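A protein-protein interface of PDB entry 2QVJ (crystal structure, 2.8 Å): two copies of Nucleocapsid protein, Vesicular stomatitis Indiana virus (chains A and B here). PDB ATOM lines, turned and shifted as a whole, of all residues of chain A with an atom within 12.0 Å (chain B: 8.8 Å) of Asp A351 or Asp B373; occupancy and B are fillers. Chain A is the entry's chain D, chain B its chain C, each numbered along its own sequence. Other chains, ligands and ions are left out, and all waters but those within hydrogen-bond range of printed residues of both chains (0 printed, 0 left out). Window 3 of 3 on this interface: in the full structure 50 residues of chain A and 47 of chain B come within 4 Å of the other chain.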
ATOM      1  N   LEU A 343      17.960   4.942 -14.431  1.00  0.00           N
ATOM      2  CA  LEU A 343      18.525   6.093 -13.742  1.00  0.00           C
ATOM      3  C   LEU A 343      17.908   6.270 -12.363  1.00  0.00           C
ATOM      4  O   LEU A 343      16.686   6.306 -12.216  1.00  0.00           O
ATOM      5  CB  LEU A 343      18.330   7.363 -14.577  1.00  0.00           C
ATOM      6  CG  LEU A 343      19.417   7.860 -15.542  1.00  0.00           C
ATOM      7  CD1 LEU A 343      20.055   6.750 -16.374  1.00  0.00           C
ATOM      8  CD2 LEU A 343      18.843   8.942 -16.446  1.00  0.00           C
ATOM      9  N   ALA A 344      18.771   6.351 -11.357  1.00  0.00           N
ATOM     10  CA  ALA A 344      18.357   6.624  -9.991  1.00  0.00           C
ATOM     11  C   ALA A 344      19.294   7.670  -9.397  1.00  0.00           C
ATOM     12  O   ALA A 344      20.466   7.751  -9.781  1.00  0.00           O
ATOM     13  CB  ALA A 344      18.383   5.351  -9.164  1.00  0.00           C
ATOM     14  N   GLN A 345      18.773   8.475  -8.476  1.00  0.00           N
ATOM     15  CA  GLN A 345      19.578   9.467  -7.778  1.00  0.00           C
ATOM     16  C   GLN A 345      20.606   8.746  -6.913  1.00  0.00           C
ATOM     17  O   GLN A 345      20.361   7.628  -6.454  1.00  0.00           O
ATOM     18  CB  GLN A 345      18.691  10.372  -6.920  1.00  0.00           C
ATOM     19  CG  GLN A 345      19.293  11.735  -6.617  1.00  0.00           C
ATOM     20  CD  GLN A 345      18.489  12.531  -5.604  1.00  0.00           C
ATOM     21  OE1 GLN A 345      17.364  12.172  -5.259  1.00  0.00           O
ATOM     22  NE2 GLN A 345      19.063  13.627  -5.124  1.00  0.00           N
ATOM     23  N   GLN A 346      21.761   9.376  -6.712  1.00  0.00           N
ATOM     24  CA  GLN A 346      22.820   8.781  -5.902  1.00  0.00           C
ATOM     25  C   GLN A 346      23.111   9.610  -4.657  1.00  0.00           C
ATOM     26  O   GLN A 346      23.197   9.071  -3.554  1.00  0.00           O
ATOM     27  CB  GLN A 346      24.097   8.582  -6.728  1.00  0.00           C
ATOM     28  CG  GLN A 346      23.948   7.664  -7.940  1.00  0.00           C
ATOM     29  CD  GLN A 346      23.578   6.239  -7.576  1.00  0.00           C
ATOM     30  OE1 GLN A 346      24.089   5.673  -6.607  1.00  0.00           O
ATOM     31  NE2 GLN A 346      22.687   5.647  -8.360  1.00  0.00           N
ATOM     32  N   PHE A 347      23.253  10.920  -4.844  1.00  0.00           N
ATOM     33  CA  PHE A 347      23.600  11.837  -3.761  1.00  0.00           C
ATOM     34  C   PHE A 347      22.599  12.979  -3.689  1.00  0.00           C
ATOM     35  O   PHE A 347      22.078  13.415  -4.719  1.00  0.00           O
ATOM     36  CB  PHE A 347      25.003  12.412  -3.977  1.00  0.00           C
ATOM     37  CG  PHE A 347      26.068  11.370  -4.170  1.00  0.00           C
ATOM     38  CD1 PHE A 347      26.762  10.856  -3.081  1.00  0.00           C
ATOM     39  CD2 PHE A 347      26.392  10.915  -5.444  1.00  0.00           C
ATOM     40  CE1 PHE A 347      27.751   9.895  -3.254  1.00  0.00           C
ATOM     41  CE2 PHE A 347      27.381   9.953  -5.627  1.00  0.00           C
ATOM     42  CZ  PHE A 347      28.061   9.441  -4.529  1.00  0.00           C
ATOM     43  N   CYS A 348      22.350  13.476  -2.477  1.00  0.00           N
ATOM     44  CA  CYS A 348      21.400  14.569  -2.270  1.00  0.00           C
ATOM     45  C   CYS A 348      21.827  15.579  -1.203  1.00  0.00           C
ATOM     46  O   CYS A 348      22.874  15.434  -0.570  1.00  0.00           O
ATOM     47  CB  CYS A 348      20.029  14.001  -1.904  1.00  0.00           C
ATOM     48  SG  CYS A 348      19.959  13.306  -0.249  1.00  0.00           S
ATOM     49  N   VAL A 349      20.991  16.599  -1.022  1.00  0.00           N
ATOM     50  CA  VAL A 349      21.114  17.567   0.070  1.00  0.00           C
ATOM     51  C   VAL A 349      19.710  18.047   0.500  1.00  0.00           C
ATOM     52  O   VAL A 349      19.239  19.110   0.076  1.00  0.00           O
ATOM     53  CB  VAL A 349      22.091  18.741  -0.292  1.00  0.00           C
ATOM     54  CG1 VAL A 349      21.827  19.288  -1.699  1.00  0.00           C
ATOM     55  CG2 VAL A 349      22.055  19.849   0.765  1.00  0.00           C
ATOM     56  N   GLY A 350      19.044  17.227   1.318  1.00  0.00           N
ATOM     57  CA  GLY A 350      17.683  17.499   1.807  1.00  0.00           C
ATOM     58  C   GLY A 350      16.561  17.494   0.773  1.00  0.00           C
ATOM     59  O   GLY A 350      15.446  17.940   1.063  1.00  0.00           O
ATOM     60  N   ASP A 351      16.847  16.985  -0.427  1.00  0.00           N
ATOM     61  CA  ASP A 351      15.902  16.980  -1.551  1.00  0.00           C
ATOM     62  C   ASP A 351      16.055  15.677  -2.341  1.00  0.00           C
ATOM     63  O   ASP A 351      16.942  15.551  -3.188  1.00  0.00           O
ATOM     64  CB  ASP A 351      16.146  18.211  -2.440  1.00  0.00           C
ATOM     65  CG  ASP A 351      15.350  18.185  -3.748  1.00  0.00           C
ATOM     66  OD1 ASP A 351      15.958  18.435  -4.810  1.00  0.00           O
ATOM     67  OD2 ASP A 351      14.125  17.935  -3.721  1.00  0.00           O
ATOM     68  N   ASN A 352      15.198  14.705  -2.038  1.00  0.00           N
ATOM     69  CA  ASN A 352      15.281  13.368  -2.632  1.00  0.00           C
ATOM     70  C   ASN A 352      14.238  13.166  -3.732  1.00  0.00           C
ATOM     71  O   ASN A 352      13.176  13.786  -3.707  1.00  0.00           O
ATOM     72  CB  ASN A 352      15.116  12.279  -1.558  1.00  0.00           C
ATOM     73  CG  ASN A 352      16.074  12.446  -0.373  1.00  0.00           C
ATOM     74  OD1 ASN A 352      16.578  13.538  -0.103  1.00  0.00           O
ATOM     75  ND2 ASN A 352      16.315  11.351   0.347  1.00  0.00           N
ATOM     76  N   LYS A 353      14.543  12.292  -4.687  1.00  0.00           N
ATOM     77  CA  LYS A 353      13.614  11.972  -5.770  1.00  0.00           C
ATOM     78  C   LYS A 353      13.028  10.575  -5.591  1.00  0.00           C
ATOM     79  O   LYS A 353      13.748   9.578  -5.621  1.00  0.00           O
ATOM     80  CB  LYS A 353      14.307  12.090  -7.134  1.00  0.00           C
ATOM     81  CG  LYS A 353      13.364  12.311  -8.317  1.00  0.00           C
ATOM     82  CD  LYS A 353      12.878  11.008  -8.943  1.00  0.00           C
ATOM     83  CE  LYS A 353      11.651  11.260  -9.802  1.00  0.00           C
ATOM     84  NZ  LYS A 353      11.227  10.053 -10.551  1.00  0.00           N
ATOM     85  N   TYR A 354      11.715  10.512  -5.401  1.00  0.00           N
ATOM     86  CA  TYR A 354      11.026   9.231  -5.329  1.00  0.00           C
ATOM     87  C   TYR A 354      10.313   8.880  -6.633  1.00  0.00           C
ATOM     88  O   TYR A 354       9.663   9.723  -7.255  1.00  0.00           O
ATOM     89  CB  TYR A 354      10.088   9.172  -4.124  1.00  0.00           C
ATOM     90  CG  TYR A 354      10.657   8.379  -2.967  1.00  0.00           C
ATOM     91  CD1 TYR A 354       9.878   7.439  -2.290  1.00  0.00           C
ATOM     92  CD2 TYR A 354      11.985   8.548  -2.561  1.00  0.00           C
ATOM     93  CE1 TYR A 354      10.398   6.698  -1.224  1.00  0.00           C
ATOM     94  CE2 TYR A 354      12.516   7.811  -1.499  1.00  0.00           C
ATOM     95  CZ  TYR A 354      11.718   6.888  -0.837  1.00  0.00           C
ATOM     96  OH  TYR A 354      12.235   6.158   0.209  1.00  0.00           O
ATOM     97  N   THR A 355      10.461   7.622  -7.032  1.00  0.00           N
ATOM     98  CA  THR A 355       9.967   7.130  -8.315  1.00  0.00           C
ATOM     99  C   THR A 355       8.786   6.136  -8.243  1.00  0.00           C
ATOM    100  O   THR A 355       8.128   5.915  -9.264  1.00  0.00           O
ATOM    101  CB  THR A 355      11.126   6.527  -9.166  1.00  0.00           C
ATOM    102  OG1 THR A 355      10.645   6.181 -10.469  1.00  0.00           O
ATOM    103  CG2 THR A 355      11.726   5.288  -8.498  1.00  0.00           C
ATOM    104  N   MET B 239      28.928  24.511 -12.224  1.00  0.00           N
ATOM    105  CA  MET B 239      28.304  24.089 -10.980  1.00  0.00           C
ATOM    106  C   MET B 239      29.358  23.750  -9.939  1.00  0.00           C
ATOM    107  O   MET B 239      30.475  23.351 -10.273  1.00  0.00           O
ATOM    108  CB  MET B 239      27.394  22.878 -11.215  1.00  0.00           C
ATOM    109  CG  MET B 239      26.364  23.069 -12.327  1.00  0.00           C
ATOM    110  SD  MET B 239      25.123  21.763 -12.357  1.00  0.00           S
ATOM    111  CE  MET B 239      24.388  22.061 -13.947  1.00  0.00           C
ATOM    112  N   ASP B 243      26.727  20.339  -6.445  1.00  0.00           N
ATOM    113  CA  ASP B 243      25.686  20.209  -7.471  1.00  0.00           C
ATOM    114  C   ASP B 243      26.030  19.126  -8.493  1.00  0.00           C
ATOM    115  O   ASP B 243      25.148  18.392  -8.951  1.00  0.00           O
ATOM    116  CB  ASP B 243      25.451  21.543  -8.195  1.00  0.00           C
ATOM    117  CG  ASP B 243      24.984  22.651  -7.266  1.00  0.00           C
ATOM    118  OD1 ASP B 243      24.110  22.399  -6.409  1.00  0.00           O
ATOM    119  OD2 ASP B 243      25.489  23.786  -7.405  1.00  0.00           O
ATOM    120  N   THR B 246      25.346  15.566  -7.076  1.00  0.00           N
ATOM    121  CA  THR B 246      23.926  15.195  -7.077  1.00  0.00           C
ATOM    122  C   THR B 246      23.465  14.664  -8.444  1.00  0.00           C
ATOM    123  O   THR B 246      22.499  13.906  -8.523  1.00  0.00           O
ATOM    124  CB  THR B 246      23.001  16.352  -6.603  1.00  0.00           C
ATOM    125  OG1 THR B 246      23.167  17.493  -7.452  1.00  0.00           O
ATOM    126  CG2 THR B 246      23.303  16.742  -5.161  1.00  0.00           C
ATOM    127  N   TRP B 247      24.180  15.044  -9.502  1.00  0.00           N
ATOM    128  CA  TRP B 247      23.858  14.626 -10.875  1.00  0.00           C
ATOM    129  C   TRP B 247      24.407  13.257 -11.303  1.00  0.00           C
ATOM    130  O   TRP B 247      24.149  12.814 -12.425  1.00  0.00           O
ATOM    131  CB  TRP B 247      24.275  15.704 -11.877  1.00  0.00           C
ATOM    132  CG  TRP B 247      23.241  16.770 -12.046  1.00  0.00           C
ATOM    133  CD1 TRP B 247      23.225  18.001 -11.455  1.00  0.00           C
ATOM    134  CD2 TRP B 247      22.062  16.699 -12.858  1.00  0.00           C
ATOM    135  NE1 TRP B 247      22.111  18.704 -11.854  1.00  0.00           N
ATOM    136  CE2 TRP B 247      21.381  17.929 -12.716  1.00  0.00           C
ATOM    137  CE3 TRP B 247      21.517  15.718 -13.701  1.00  0.00           C
ATOM    138  CZ2 TRP B 247      20.183  18.202 -13.379  1.00  0.00           C
ATOM    139  CZ3 TRP B 247      20.323  15.991 -14.360  1.00  0.00           C
ATOM    140  CH2 TRP B 247      19.671  17.223 -14.195  1.00  0.00           C
ATOM    141  N   LEU B 332      21.295  13.635 -20.570  1.00  0.00           N
ATOM    142  CA  LEU B 332      20.253  14.262 -19.753  1.00  0.00           C
ATOM    143  C   LEU B 332      20.804  15.465 -19.004  1.00  0.00           C
ATOM    144  O   LEU B 332      20.144  16.501 -18.900  1.00  0.00           O
ATOM    145  CB  LEU B 332      19.663  13.258 -18.755  1.00  0.00           C
ATOM    146  CG  LEU B 332      18.570  13.746 -17.790  1.00  0.00           C
ATOM    147  CD1 LEU B 332      17.227  13.914 -18.497  1.00  0.00           C
ATOM    148  CD2 LEU B 332      18.429  12.799 -16.616  1.00  0.00           C
ATOM    149  N   TYR B 333      22.026  15.307 -18.499  1.00  0.00           N
ATOM    150  CA  TYR B 333      22.704  16.318 -17.704  1.00  0.00           C
ATOM    151  C   TYR B 333      23.171  17.460 -18.598  1.00  0.00           C
ATOM    152  O   TYR B 333      22.914  18.626 -18.298  1.00  0.00           O
ATOM    153  CB  TYR B 333      23.873  15.672 -16.945  1.00  0.00           C
ATOM    154  CG  TYR B 333      24.647  16.568 -15.992  1.00  0.00           C
ATOM    155  CD1 TYR B 333      24.042  17.658 -15.354  1.00  0.00           C
ATOM    156  CD2 TYR B 333      25.984  16.292 -15.696  1.00  0.00           C
ATOM    157  CE1 TYR B 333      24.762  18.464 -14.473  1.00  0.00           C
ATOM    158  CE2 TYR B 333      26.712  17.090 -14.814  1.00  0.00           C
ATOM    159  CZ  TYR B 333      26.097  18.170 -14.207  1.00  0.00           C
ATOM    160  OH  TYR B 333      26.820  18.949 -13.338  1.00  0.00           O
ATOM    161  N   ALA B 336      20.421  19.422 -19.728  1.00  0.00           N
ATOM    162  CA  ALA B 336      19.894  20.232 -18.631  1.00  0.00           C
ATOM    163  C   ALA B 336      20.653  21.545 -18.428  1.00  0.00           C
ATOM    164  O   ALA B 336      20.062  22.532 -17.997  1.00  0.00           O
ATOM    165  CB  ALA B 336      19.856  19.427 -17.335  1.00  0.00           C
ATOM    166  N   VAL B 337      21.951  21.562 -18.728  1.00  0.00           N
ATOM    167  CA  VAL B 337      22.739  22.793 -18.580  1.00  0.00           C
ATOM    168  C   VAL B 337      22.818  23.580 -19.896  1.00  0.00           C
ATOM    169  O   VAL B 337      23.008  24.801 -19.890  1.00  0.00           O
ATOM    170  CB  VAL B 337      24.155  22.559 -17.931  1.00  0.00           C
ATOM    171  CG1 VAL B 337      24.255  21.180 -17.297  1.00  0.00           C
ATOM    172  CG2 VAL B 337      25.284  22.763 -18.923  1.00  0.00           C
ATOM    173  N   SER B 340      19.387  25.243 -20.200  1.00  0.00           N
ATOM    174  CA  SER B 340      19.215  26.150 -19.066  1.00  0.00           C
ATOM    175  C   SER B 340      20.498  26.932 -18.797  1.00  0.00           C
ATOM    176  O   SER B 340      21.341  26.515 -17.995  1.00  0.00           O
ATOM    177  CB  SER B 340      18.768  25.388 -17.812  1.00  0.00           C
ATOM    178  OG  SER B 340      17.512  24.759 -18.009  1.00  0.00           O
ATOM    179  N   ASP B 342      20.683  29.945 -17.403  1.00  0.00           N
ATOM    180  CA  ASP B 342      20.560  30.622 -16.106  1.00  0.00           C
ATOM    181  C   ASP B 342      21.326  31.944 -16.079  1.00  0.00           C
ATOM    182  O   ASP B 342      22.105  32.215 -15.162  1.00  0.00           O
ATOM    183  CB  ASP B 342      20.976  29.702 -14.949  1.00  0.00           C
ATOM    184  CG  ASP B 342      20.048  28.516 -14.789  1.00  0.00           C
ATOM    185  OD1 ASP B 342      18.879  28.720 -14.399  1.00  0.00           O
ATOM    186  OD2 ASP B 342      20.487  27.378 -15.054  1.00  0.00           O
ATOM    187  N   PRO B 369      12.268  21.394 -17.069  1.00  0.00           N
ATOM    188  CA  PRO B 369      12.490  22.278 -15.920  1.00  0.00           C
ATOM    189  C   PRO B 369      13.371  23.477 -16.258  1.00  0.00           C
ATOM    190  O   PRO B 369      14.219  23.393 -17.147  1.00  0.00           O
ATOM    191  CB  PRO B 369      13.213  21.375 -14.917  1.00  0.00           C
ATOM    192  CG  PRO B 369      12.806  20.004 -15.280  1.00  0.00           C
ATOM    193  CD  PRO B 369      12.664  20.005 -16.767  1.00  0.00           C
ATOM    194  N   GLN B 370      13.167  24.578 -15.543  1.00  0.00           N
ATOM    195  CA  GLN B 370      13.908  25.811 -15.797  1.00  0.00           C
ATOM    196  C   GLN B 370      15.303  25.795 -15.181  1.00  0.00           C
ATOM    197  O   GLN B 370      16.246  26.334 -15.762  1.00  0.00           O
ATOM    198  CB  GLN B 370      13.123  27.032 -15.305  1.00  0.00           C
ATOM    199  CG  GLN B 370      11.790  27.262 -16.018  1.00  0.00           C
ATOM    200  CD  GLN B 370      11.926  27.341 -17.532  1.00  0.00           C
ATOM    201  OE1 GLN B 370      12.745  28.099 -18.061  1.00  0.00           O
ATOM    202  NE2 GLN B 370      11.116  26.556 -18.237  1.00  0.00           N
ATOM    203  N   GLY B 371      15.429  25.173 -14.012  1.00  0.00           N
ATOM    204  CA  GLY B 371      16.693  25.160 -13.283  1.00  0.00           C
ATOM    205  C   GLY B 371      17.644  24.046 -13.679  1.00  0.00           C
ATOM    206  O   GLY B 371      17.656  23.592 -14.825  1.00  0.00           O
ATOM    207  N   ARG B 372      18.454  23.621 -12.714  1.00  0.00           N
ATOM    208  CA  ARG B 372      19.406  22.534 -12.897  1.00  0.00           C
ATOM    209  C   ARG B 372      19.280  21.525 -11.751  1.00  0.00           C
ATOM    210  O   ARG B 372      20.231  20.814 -11.417  1.00  0.00           O
ATOM    211  CB  ARG B 372      20.829  23.090 -12.998  1.00  0.00           C
ATOM    212  CG  ARG B 372      21.083  23.895 -14.264  1.00  0.00           C
ATOM    213  CD  ARG B 372      22.350  24.731 -14.173  1.00  0.00           C
ATOM    214  NE  ARG B 372      22.709  25.284 -15.477  1.00  0.00           N
ATOM    215  CZ  ARG B 372      23.860  25.887 -15.759  1.00  0.00           C
ATOM    216  NH1 ARG B 372      24.795  26.027 -14.831  1.00  0.00           N
ATOM    217  NH2 ARG B 372      24.075  26.352 -16.982  1.00  0.00           N
ATOM    218  N   ASP B 373      18.091  21.470 -11.158  1.00  0.00           N
ATOM    219  CA  ASP B 373      17.805  20.544 -10.072  1.00  0.00           C
ATOM    220  C   ASP B 373      17.555  19.135 -10.605  1.00  0.00           C
ATOM    221  O   ASP B 373      16.717  18.937 -11.487  1.00  0.00           O
ATOM    222  CB  ASP B 373      16.599  21.025  -9.263  1.00  0.00           C
ATOM    223  CG  ASP B 373      16.322  20.151  -8.055  1.00  0.00           C
ATOM    224  OD1 ASP B 373      17.291  19.771  -7.364  1.00  0.00           O
ATOM    225  OD2 ASP B 373      15.139  19.844  -7.793  1.00  0.00           O
ATOM    226  N   VAL B 374      18.277  18.166 -10.048  1.00  0.00           N
ATOM    227  CA  VAL B 374      18.215  16.769 -10.492  1.00  0.00           C
ATOM    228  C   VAL B 374      16.847  16.134 -10.249  1.00  0.00           C
ATOM    229  O   VAL B 374      16.357  15.364 -11.075  1.00  0.00           O
ATOM    230  CB  VAL B 374      19.278  15.896  -9.792  1.00  0.00           C
ATOM    231  CG1 VAL B 374      19.675  14.731 -10.684  1.00  0.00           C
ATOM    232  CG2 VAL B 374      20.501  16.722  -9.423  1.00  0.00           C
ATOM    233  N   VAL B 375      16.241  16.463  -9.110  1.00  0.00           N
ATOM    234  CA  VAL B 375      14.947  15.905  -8.726  1.00  0.00           C
ATOM    235  C   VAL B 375      13.845  16.398  -9.668  1.00  0.00           C
ATOM    236  O   VAL B 375      12.960  15.630 -10.053  1.00  0.00           O
ATOM    237  CB  VAL B 375      14.625  16.199  -7.240  1.00  0.00           C
ATOM    238  CG1 VAL B 375      13.255  15.665  -6.852  1.00  0.00           C
ATOM    239  CG2 VAL B 375      15.697  15.585  -6.346  1.00  0.00           C
ATOM    240  N   GLU B 376      13.916  17.670 -10.052  1.00  0.00           N
ATOM    241  CA  GLU B 376      13.000  18.215 -11.049  1.00  0.00           C
ATOM    242  C   GLU B 376      13.170  17.500 -12.388  1.00  0.00           C
ATOM    243  O   GLU B 376      12.187  17.095 -13.011  1.00  0.00           O
ATOM    244  CB  GLU B 376      13.206  19.721 -11.219  1.00  0.00           C
ATOM    245  CG  GLU B 376      12.493  20.580 -10.180  1.00  0.00           C
ATOM    246  CD  GLU B 376      12.787  22.073 -10.329  1.00  0.00           C
ATOM    247  OE1 GLU B 376      13.766  22.439 -11.018  1.00  0.00           O
ATOM    248  OE2 GLU B 376      12.040  22.886  -9.748  1.00  0.00           O
ATOM    249  N   TRP B 377      14.423  17.331 -12.810  1.00  0.00           N
ATOM    250  CA  TRP B 377      14.733  16.692 -14.091  1.00  0.00           C
ATOM    251  C   TRP B 377      14.444  15.187 -14.134  1.00  0.00           C
ATOM    252  O   TRP B 377      13.994  14.677 -15.161  1.00  0.00           O
ATOM    253  CB  TRP B 377      16.171  16.991 -14.519  1.00  0.00           C
ATOM    254  CG  TRP B 377      16.346  18.390 -15.062  1.00  0.00           C
ATOM    255  CD1 TRP B 377      16.676  19.511 -14.352  1.00  0.00           C
ATOM    256  CD2 TRP B 377      16.189  18.812 -16.424  1.00  0.00           C
ATOM    257  NE1 TRP B 377      16.737  20.602 -15.185  1.00  0.00           N
ATOM    258  CE2 TRP B 377      16.441  20.202 -16.461  1.00  0.00           C
ATOM    259  CE3 TRP B 377      15.861  18.150 -17.614  1.00  0.00           C
ATOM    260  CZ2 TRP B 377      16.379  20.945 -17.647  1.00  0.00           C
ATOM    261  CZ3 TRP B 377      15.795  18.891 -18.792  1.00  0.00           C
ATOM    262  CH2 TRP B 377      16.055  20.273 -18.797  1.00  0.00           C
ATOM    263  N   LEU B 378      14.689  14.485 -13.028  1.00  0.00           N
ATOM    264  CA  LEU B 378      14.374  13.051 -12.934  1.00  0.00           C
ATOM    265  C   LEU B 378      12.874  12.780 -12.973  1.00  0.00           C
ATOM    266  O   LEU B 378      12.434  11.795 -13.571  1.00  0.00           O
ATOM    267  CB  LEU B 378      14.985  12.428 -11.675  1.00  0.00           C
ATOM    268  CG  LEU B 378      16.438  11.950 -11.754  1.00  0.00           C
ATOM    269  CD1 LEU B 378      17.059  11.916 -10.369  1.00  0.00           C
ATOM    270  CD2 LEU B 378      16.534  10.585 -12.426  1.00  0.00           C
ATOM    271  N   GLY B 379      12.100  13.653 -12.328  1.00  0.00           N
ATOM    272  CA  GLY B 379      10.639  13.579 -12.350  1.00  0.00           C
ATOM    273  C   GLY B 379      10.088  13.955 -13.711  1.00  0.00           C
ATOM    274  O   GLY B 379       9.091  13.392 -14.163  1.00  0.00           O
ATOM    275  N   TRP B 380      10.743  14.911 -14.364  1.00  0.00           N
ATOM    276  CA  TRP B 380      10.392  15.292 -15.726  1.00  0.00           C
ATOM    277  C   TRP B 380      10.713  14.172 -16.716  1.00  0.00           C
ATOM    278  O   TRP B 380       9.914  13.880 -17.601  1.00  0.00           O
ATOM    279  CB  TRP B 380      11.106  16.582 -16.137  1.00  0.00           C
ATOM    280  CG  TRP B 380      10.890  16.924 -17.576  1.00  0.00           C
ATOM    281  CD1 TRP B 380       9.832  17.601 -18.111  1.00  0.00           C
ATOM    282  CD2 TRP B 380      11.745  16.584 -18.675  1.00  0.00           C
ATOM    283  NE1 TRP B 380       9.979  17.711 -19.472  1.00  0.00           N
ATOM    284  CE2 TRP B 380      11.145  17.097 -19.846  1.00  0.00           C
ATOM    285  CE3 TRP B 380      12.961  15.894 -18.782  1.00  0.00           C
ATOM    286  CZ2 TRP B 380      11.717  16.946 -21.109  1.00  0.00           C
ATOM    287  CZ3 TRP B 380      13.533  15.745 -20.041  1.00  0.00           C
ATOM    288  CH2 TRP B 380      12.910  16.270 -21.188  1.00  0.00           C
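OD1 of Asp A351 lies close to OD1 of Asp B373 (3.2 Å).
The side-chain carboxylate (OD2) of Asp B373 lies within hydrogen-bond range of the backbone NH (N) of Glu B376 (3.4 Å).
The side-chain amide oxygen (OE1) of Gln A345 lies within hydrogen-bond range of the backbone NH (N) of Lys A353, 2.9 Å away.
SG of Cys A348 lies within hydrogen-bond range of OD1 of Asn A352, at 3.4 Å.
The side-chain hydroxyl (OG1) of Thr B246 is in hydrogen-bond range of the backbone carbonyl oxygen (O) of Asp B243, 2.6 Å away.
NE2 of Gln A345 lies within hydrogen-bond range of O of Asp A351, 3.5 Å away.
The backbone carbonyl oxygen (O) of Phe A347 lies within hydrogen-bond range of the side-chain amide nitrogen (NE2) of Gln A345, 3.0 Å away.
No position is printed for both chains.
Of the 9 pairs that touch across the chains among the printed residues, none has its exchanged pair printed and touching as well.
Among the printed residues, merely in contact across the chains: Leu A343 with Leu B332 (3.9 Å), Gln A345 with Val B375 (3.95 Å), Phe A347 with Thr B246 (3.5 Å), Asp A351 with Val B375 (3.2 Å), Asn A352 with Val B375 (3.7 Å), Lys A353 with Val B375 (3.7 Å), Lys A353 with Leu B378 (3.7 Å) and Lys A353 with Gly B379 (3.5 Å).
Printed residues of chain B within 4 Å of Phe A347: Thr B246 (3.5 Å).
No residue of chain B comes within 4 Å of Gly A350.
Asp A351 touches two residues of chain B.
Of the printed residues of chain B, Asn A352 touches Val B375 (3.7 Å).
Met B239 touches none of the printed residues of chain A.
Ser B340 touches none of the printed residues of chain A.
Pro B369 touches none of the printed residues of chain A.
Asp B373 touches just one residue of chain A: Asp A351.
No residue of chain A comes within 4 Å of Glu B376.
Printed residues of chain A within 4 Å of Gly B379: Lys A353 (3.5 Å).
The nearest residue of chain A that does not touch Asp B373 is Gln A345 (6.8 Å).
Of the 22 printed residues of chain B, 6 touch a printed residue of chain A.
Hydrophobic or aromatic side chains of chain B within 4 Å of the printed part of chain A: Leu B332, Val B375 and Leu B378.
Along chain B the printed residues that touch a printed residue of chain A span positions 246 to 379.
Among the printed residues, 9 pairs touch across the chains.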
